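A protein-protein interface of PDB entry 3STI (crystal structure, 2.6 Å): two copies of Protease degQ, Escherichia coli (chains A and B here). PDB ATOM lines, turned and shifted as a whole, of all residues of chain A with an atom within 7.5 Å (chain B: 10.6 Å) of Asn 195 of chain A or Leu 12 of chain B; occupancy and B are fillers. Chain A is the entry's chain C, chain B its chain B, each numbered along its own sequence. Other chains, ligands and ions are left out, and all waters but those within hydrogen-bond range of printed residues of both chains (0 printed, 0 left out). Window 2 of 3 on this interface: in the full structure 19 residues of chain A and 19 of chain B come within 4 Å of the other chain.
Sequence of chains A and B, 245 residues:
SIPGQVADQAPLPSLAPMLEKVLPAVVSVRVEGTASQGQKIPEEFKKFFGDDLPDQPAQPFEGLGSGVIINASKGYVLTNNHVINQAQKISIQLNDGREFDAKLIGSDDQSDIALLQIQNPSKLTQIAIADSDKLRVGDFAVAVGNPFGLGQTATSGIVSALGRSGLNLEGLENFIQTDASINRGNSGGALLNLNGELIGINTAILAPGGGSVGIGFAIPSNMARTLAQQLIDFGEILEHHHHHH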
ATOM      1  N   MET A  18     -20.909  11.926  12.050  1.00  0.00           N
ATOM      2  CA  MET A  18     -20.739  10.482  12.022  1.00  0.00           C
ATOM      3  C   MET A  18     -21.613   9.842  10.900  1.00  0.00           C
ATOM      4  O   MET A  18     -21.203   8.839  10.311  1.00  0.00           O
ATOM      5  CB  MET A  18     -20.963   9.860  13.408  1.00  0.00           C
ATOM      6  CG  MET A  18     -22.390   9.561  13.758  1.00  0.00           C
ATOM      7  SD  MET A  18     -22.857   7.888  13.284  1.00  0.00           S
ATOM      8  CE  MET A  18     -24.283   7.719  14.250  1.00  0.00           C
ATOM      9  N   LYS A  21     -19.797   9.665   7.241  1.00  0.00           N
ATOM     10  CA  LYS A  21     -18.818   8.613   7.007  1.00  0.00           C
ATOM     11  C   LYS A  21     -19.469   7.251   6.727  1.00  0.00           C
ATOM     12  O   LYS A  21     -18.900   6.449   5.990  1.00  0.00           O
ATOM     13  CB  LYS A  21     -17.868   8.497   8.190  1.00  0.00           C
ATOM     14  CG  LYS A  21     -17.019   9.717   8.380  1.00  0.00           C
ATOM     15  CD  LYS A  21     -15.905   9.419   9.358  1.00  0.00           C
ATOM     16  CE  LYS A  21     -14.817  10.448   9.264  1.00  0.00           C
ATOM     17  NZ  LYS A  21     -13.599  10.030  10.016  1.00  0.00           N
ATOM     18  N   VAL A  22     -20.675   7.019   7.266  1.00  0.00           N
ATOM     19  CA  VAL A  22     -21.469   5.785   7.171  1.00  0.00           C
ATOM     20  C   VAL A  22     -22.365   5.743   5.903  1.00  0.00           C
ATOM     21  O   VAL A  22     -22.749   4.659   5.464  1.00  0.00           O
ATOM     22  CB  VAL A  22     -22.307   5.682   8.474  1.00  0.00           C
ATOM     23  CG1 VAL A  22     -23.473   4.704   8.356  1.00  0.00           C
ATOM     24  CG2 VAL A  22     -21.420   5.333   9.660  1.00  0.00           C
ATOM     25  N   ALA A 128     -18.345  -0.677   9.439  1.00  0.00           N
ATOM     26  CA  ALA A 128     -17.606  -1.282  10.542  1.00  0.00           C
ATOM     27  C   ALA A 128     -18.654  -1.946  11.416  1.00  0.00           C
ATOM     28  O   ALA A 128     -19.762  -1.412  11.504  1.00  0.00           O
ATOM     29  CB  ALA A 128     -16.829  -0.220  11.309  1.00  0.00           C
ATOM     30  N   ALA A 130     -19.740  -3.704  15.181  1.00  0.00           N
ATOM     31  CA  ALA A 130     -19.456  -3.707  16.607  1.00  0.00           C
ATOM     32  C   ALA A 130     -19.986  -4.989  17.268  1.00  0.00           C
ATOM     33  O   ALA A 130     -20.916  -5.626  16.746  1.00  0.00           O
ATOM     34  CB  ALA A 130     -20.087  -2.481  17.253  1.00  0.00           C
ATOM     35  N   ARG A 136     -25.492  -2.255  26.229  1.00  0.00           N
ATOM     36  CA  ARG A 136     -26.151  -2.025  27.513  1.00  0.00           C
ATOM     37  C   ARG A 136     -27.341  -1.128  27.307  1.00  0.00           C
ATOM     38  O   ARG A 136     -27.258  -0.200  26.503  1.00  0.00           O
ATOM     39  CB  ARG A 136     -25.191  -1.366  28.525  1.00  0.00           C
ATOM     40  CG  ARG A 136     -23.967  -2.196  28.939  1.00  0.00           C
ATOM     41  CD  ARG A 136     -23.146  -1.503  30.014  1.00  0.00           C
ATOM     42  NE  ARG A 136     -22.579  -0.235  29.542  1.00  0.00           N
ATOM     43  CZ  ARG A 136     -22.019   0.683  30.327  1.00  0.00           C
ATOM     44  NH1 ARG A 136     -21.925   0.481  31.637  1.00  0.00           N
ATOM     45  NH2 ARG A 136     -21.551   1.812  29.809  1.00  0.00           N
ATOM     46  N   ASP A 139     -27.434   2.805  26.113  1.00  0.00           N
ATOM     47  CA  ASP A 139     -26.475   3.173  25.053  1.00  0.00           C
ATOM     48  C   ASP A 139     -27.212   3.878  23.927  1.00  0.00           C
ATOM     49  O   ASP A 139     -28.337   3.494  23.604  1.00  0.00           O
ATOM     50  CB  ASP A 139     -25.716   1.949  24.498  1.00  0.00           C
ATOM     51  CG  ASP A 139     -24.683   1.329  25.426  1.00  0.00           C
ATOM     52  OD1 ASP A 139     -24.055   2.080  26.216  1.00  0.00           O
ATOM     53  OD2 ASP A 139     -24.478   0.101  25.344  1.00  0.00           O
ATOM     54  N   PHE A 140     -26.603   4.909  23.342  1.00  0.00           N
ATOM     55  CA  PHE A 140     -27.258   5.667  22.279  1.00  0.00           C
ATOM     56  C   PHE A 140     -27.251   4.897  20.951  1.00  0.00           C
ATOM     57  O   PHE A 140     -26.275   4.215  20.623  1.00  0.00           O
ATOM     58  CB  PHE A 140     -26.625   7.058  22.131  1.00  0.00           C
ATOM     59  CG  PHE A 140     -26.840   7.938  23.346  1.00  0.00           C
ATOM     60  CD1 PHE A 140     -25.804   8.195  24.226  1.00  0.00           C
ATOM     61  CD2 PHE A 140     -28.091   8.476  23.625  1.00  0.00           C
ATOM     62  CE1 PHE A 140     -26.007   8.990  25.361  1.00  0.00           C
ATOM     63  CE2 PHE A 140     -28.295   9.275  24.756  1.00  0.00           C
ATOM     64  CZ  PHE A 140     -27.250   9.530  25.619  1.00  0.00           C
ATOM     65  N   LEU A 192     -26.993   2.071  14.484  1.00  0.00           N
ATOM     66  CA  LEU A 192     -25.584   2.385  14.779  1.00  0.00           C
ATOM     67  C   LEU A 192     -25.328   2.978  16.140  1.00  0.00           C
ATOM     68  O   LEU A 192     -26.187   3.663  16.701  1.00  0.00           O
ATOM     69  CB  LEU A 192     -25.015   3.420  13.769  1.00  0.00           C
ATOM     70  CG  LEU A 192     -25.309   3.287  12.294  1.00  0.00           C
ATOM     71  CD1 LEU A 192     -25.209   4.628  11.645  1.00  0.00           C
ATOM     72  CD2 LEU A 192     -24.387   2.293  11.632  1.00  0.00           C
ATOM     73  N   ASN A 193     -24.079   2.838  16.606  1.00  0.00           N
ATOM     74  CA  ASN A 193     -23.674   3.493  17.837  1.00  0.00           C
ATOM     75  C   ASN A 193     -23.140   4.879  17.435  1.00  0.00           C
ATOM     76  O   ASN A 193     -23.217   5.232  16.256  1.00  0.00           O
ATOM     77  CB  ASN A 193     -22.664   2.646  18.659  1.00  0.00           C
ATOM     78  CG  ASN A 193     -21.381   2.235  17.977  1.00  0.00           C
ATOM     79  OD1 ASN A 193     -20.907   2.847  17.014  1.00  0.00           O
ATOM     80  ND2 ASN A 193     -20.753   1.199  18.515  1.00  0.00           N
ATOM     81  N   LEU A 194     -22.613   5.653  18.393  1.00  0.00           N
ATOM     82  CA  LEU A 194     -22.092   6.998  18.158  1.00  0.00           C
ATOM     83  C   LEU A 194     -20.766   6.978  17.368  1.00  0.00           C
ATOM     84  O   LEU A 194     -20.316   8.032  16.930  1.00  0.00           O
ATOM     85  CB  LEU A 194     -21.924   7.755  19.494  1.00  0.00           C
ATOM     86  CG  LEU A 194     -23.220   8.112  20.256  1.00  0.00           C
ATOM     87  CD1 LEU A 194     -22.963   8.213  21.740  1.00  0.00           C
ATOM     88  CD2 LEU A 194     -23.848   9.401  19.734  1.00  0.00           C
ATOM     89  N   ASN A 195     -20.147   5.793  17.173  1.00  0.00           N
ATOM     90  CA  ASN A 195     -18.900   5.627  16.408  1.00  0.00           C
ATOM     91  C   ASN A 195     -19.202   5.341  14.933  1.00  0.00           C
ATOM     92  O   ASN A 195     -18.310   5.456  14.095  1.00  0.00           O
ATOM     93  CB  ASN A 195     -18.032   4.504  16.990  1.00  0.00           C
ATOM     94  CG  ASN A 195     -17.181   4.896  18.161  1.00  0.00           C
ATOM     95  OD1 ASN A 195     -16.580   5.978  18.204  1.00  0.00           O
ATOM     96  ND2 ASN A 195     -17.082   3.999  19.125  1.00  0.00           N
ATOM     97  N   GLY A 196     -20.446   4.984  14.639  1.00  0.00           N
ATOM     98  CA  GLY A 196     -20.907   4.685  13.289  1.00  0.00           C
ATOM     99  C   GLY A 196     -20.730   3.230  12.921  1.00  0.00           C
ATOM    100  O   GLY A 196     -20.721   2.886  11.739  1.00  0.00           O
ATOM    101  N   GLU A 197     -20.592   2.373  13.946  1.00  0.00           N
ATOM    102  CA  GLU A 197     -20.414   0.924  13.820  1.00  0.00           C
ATOM    103  C   GLU A 197     -21.747   0.239  13.966  1.00  0.00           C
ATOM    104  O   GLU A 197     -22.536   0.623  14.832  1.00  0.00           O
ATOM    105  CB  GLU A 197     -19.422   0.390  14.874  1.00  0.00           C
ATOM    106  CG  GLU A 197     -18.056   1.037  14.843  1.00  0.00           C
ATOM    107  CD  GLU A 197     -17.274   0.927  16.132  1.00  0.00           C
ATOM    108  OE1 GLU A 197     -16.025   0.977  16.071  1.00  0.00           O
ATOM    109  OE2 GLU A 197     -17.907   0.825  17.208  1.00  0.00           O
ATOM    110  N   LEU A 198     -21.990  -0.793  13.151  1.00  0.00           N
ATOM    111  CA  LEU A 198     -23.237  -1.550  13.130  1.00  0.00           C
ATOM    112  C   LEU A 198     -23.443  -2.338  14.441  1.00  0.00           C
ATOM    113  O   LEU A 198     -22.579  -3.112  14.857  1.00  0.00           O
ATOM    114  CB  LEU A 198     -23.249  -2.495  11.910  1.00  0.00           C
ATOM    115  CG  LEU A 198     -24.568  -3.199  11.595  1.00  0.00           C
ATOM    116  CD1 LEU A 198     -25.444  -2.351  10.682  1.00  0.00           C
ATOM    117  CD2 LEU A 198     -24.322  -4.537  10.946  1.00  0.00           C
ATOM    118  N   PRO B  11     -14.025   5.903  24.607  1.00  0.00           N
ATOM    119  CA  PRO B  11     -15.152   5.899  25.551  1.00  0.00           C
ATOM    120  C   PRO B  11     -16.304   6.780  25.045  1.00  0.00           C
ATOM    121  O   PRO B  11     -16.140   7.990  24.795  1.00  0.00           O
ATOM    122  CB  PRO B  11     -14.537   6.430  26.856  1.00  0.00           C
ATOM    123  CG  PRO B  11     -13.235   7.159  26.437  1.00  0.00           C
ATOM    124  CD  PRO B  11     -13.015   6.928  24.948  1.00  0.00           C
ATOM    125  N   LEU B  12     -17.476   6.143  24.887  1.00  0.00           N
ATOM    126  CA  LEU B  12     -18.703   6.769  24.390  1.00  0.00           C
ATOM    127  C   LEU B  12     -19.649   7.195  25.506  1.00  0.00           C
ATOM    128  O   LEU B  12     -19.829   6.430  26.459  1.00  0.00           O
ATOM    129  CB  LEU B  12     -19.471   5.801  23.457  1.00  0.00           C
ATOM    130  CG  LEU B  12     -18.844   5.424  22.113  1.00  0.00           C
ATOM    131  CD1 LEU B  12     -19.754   4.479  21.355  1.00  0.00           C
ATOM    132  CD2 LEU B  12     -18.524   6.660  21.258  1.00  0.00           C
ATOM    133  N   PRO B  13     -20.333   8.358  25.379  1.00  0.00           N
ATOM    134  CA  PRO B  13     -21.330   8.720  26.403  1.00  0.00           C
ATOM    135  C   PRO B  13     -22.532   7.774  26.304  1.00  0.00           C
ATOM    136  O   PRO B  13     -22.853   7.268  25.218  1.00  0.00           O
ATOM    137  CB  PRO B  13     -21.685  10.178  26.071  1.00  0.00           C
ATOM    138  CG  PRO B  13     -21.399  10.319  24.608  1.00  0.00           C
ATOM    139  CD  PRO B  13     -20.274   9.358  24.291  1.00  0.00           C
ATOM    140  N   SER B  14     -23.149   7.486  27.457  1.00  0.00           N
ATOM    141  CA  SER B  14     -24.257   6.544  27.604  1.00  0.00           C
ATOM    142  C   SER B  14     -25.084   6.884  28.824  1.00  0.00           C
ATOM    143  O   SER B  14     -24.612   7.601  29.712  1.00  0.00           O
ATOM    144  CB  SER B  14     -23.701   5.131  27.748  1.00  0.00           C
ATOM    145  OG  SER B  14     -24.729   4.159  27.824  1.00  0.00           O
ATOM    146  N   LEU B  15     -26.319   6.379  28.867  1.00  0.00           N
ATOM    147  CA  LEU B  15     -27.226   6.553  30.002  1.00  0.00           C
ATOM    148  C   LEU B  15     -27.147   5.306  30.900  1.00  0.00           C
ATOM    149  O   LEU B  15     -27.712   5.301  31.990  1.00  0.00           O
ATOM    150  CB  LEU B  15     -28.677   6.817  29.537  1.00  0.00           C
ATOM    151  CG  LEU B  15     -28.972   8.134  28.825  1.00  0.00           C
ATOM    152  CD1 LEU B  15     -30.383   8.126  28.238  1.00  0.00           C
ATOM    153  CD2 LEU B  15     -28.828   9.317  29.763  1.00  0.00           C
ATOM    154  N   ALA B  16     -26.417   4.267  30.443  1.00  0.00           N
ATOM    155  CA  ALA B  16     -26.187   2.999  31.144  1.00  0.00           C
ATOM    156  C   ALA B  16     -25.471   3.196  32.503  1.00  0.00           C
ATOM    157  O   ALA B  16     -25.915   2.558  33.457  1.00  0.00           O
ATOM    158  CB  ALA B  16     -25.405   2.024  30.268  1.00  0.00           C
ATOM    159  N   PRO B  17     -24.443   4.076  32.672  1.00  0.00           N
ATOM    160  CA  PRO B  17     -23.829   4.231  34.011  1.00  0.00           C
ATOM    161  C   PRO B  17     -24.786   4.726  35.108  1.00  0.00           C
ATOM    162  O   PRO B  17     -24.634   4.306  36.252  1.00  0.00           O
ATOM    163  CB  PRO B  17     -22.706   5.249  33.775  1.00  0.00           C
ATOM    164  CG  PRO B  17     -22.401   5.146  32.308  1.00  0.00           C
ATOM    165  CD  PRO B  17     -23.740   4.919  31.679  1.00  0.00           C
ATOM    166  N   MET B  18     -25.771   5.584  34.788  1.00  0.00           N
ATOM    167  CA  MET B  18     -26.701   6.022  35.825  1.00  0.00           C
ATOM    168  C   MET B  18     -27.838   4.974  36.011  1.00  0.00           C
ATOM    169  O   MET B  18     -28.344   4.823  37.127  1.00  0.00           O
ATOM    170  CB  MET B  18     -27.231   7.453  35.575  1.00  0.00           C
ATOM    171  CG  MET B  18     -28.374   7.568  34.605  1.00  0.00           C
ATOM    172  SD  MET B  18     -29.978   7.496  35.440  1.00  0.00           S
ATOM    173  CE  MET B  18     -31.015   8.100  34.141  1.00  0.00           C
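Printed residues of chain B within 4 Å of Arg 136 of chain A: Ala 16 (3.6 Å).
Of the printed residues of chain B, Phe 140 of chain A touches Pro 13 (3.2 Å), Ser 14 (3.8 Å) and Leu 15 (3.9 Å).
No residue of chain B comes within 4 Å of Asn 193 of chain A.
Asn 195 of chain A touches just one residue of chain B: Leu 12.
No residue of chain B comes within 4 Å of Gly 196 of chain A.
No residue of chain B comes within 4 Å of Glu 197 of chain A.
Leu 198 of chain A touches none of the printed residues of chain B.
Pro 11 of chain B touches none of the printed residues of chain A.
Of the printed residues of chain A, Leu 12 of chain B touches Leu 194 (3.98 Å) and Asn 195 (3.5 Å).
Of the printed residues of chain A, Ser 14 of chain B touches Asp 139 (2.7 Å) and Phe 140 (3.8 Å).
The nearest printed residue of chain A that does not touch Leu 12 of chain B is Asn 193 of chain A (4.4 Å).
Of the 15 printed residues of chain A, 5 touch a printed residue of chain B.
Hydrophobic or aromatic side chains of chain A that line the printed part of chain B: Phe 140 and Leu 194.
Among the printed residues, 8 pairs touch across the chains.
Position printed for both chains: 18.
The side-chain carboxylate (OD1) of Asp 139 of chain A is in hydrogen-bond range of the side-chain hydroxyl (OG) of Ser 14 of chain B.
Arg 136 of chain A touches Ala 16 of chain B (CZ to CB, 3.6 Å).
Pro 13 of chain B touches Phe 140 of chain A (O to CD1, 3.2 Å).
Ser 14 of chain B touches Phe 140 of chain A (CA to CE1, 3.8 Å).
CZ of Phe 140 of chain A touches CG of Leu 15 of chain B, at 3.9 Å.
Leu 194 of chain A touches Leu 12 of chain B (CB to CD2, 3.98 Å).
CD1 of Leu 194 of chain A touches O of Pro 13 of chain B, 3.6 Å away.
Asn 195 of chain A touches Leu 12 of chain B.
N of Ala 16 of chain B lies within hydrogen-bond range of OG of Ser 14 of chain B (3.1 Å).
The backbone NH (N) of Arg 136 of chain A is in hydrogen-bond range of the side-chain carboxylate (OD2) of Asp 139 of chain A (2.7 Å).
The backbone NH of Asn 195 of chain A lies within hydrogen-bond range of the side-chain amide oxygen of Asn 193 of chain A.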
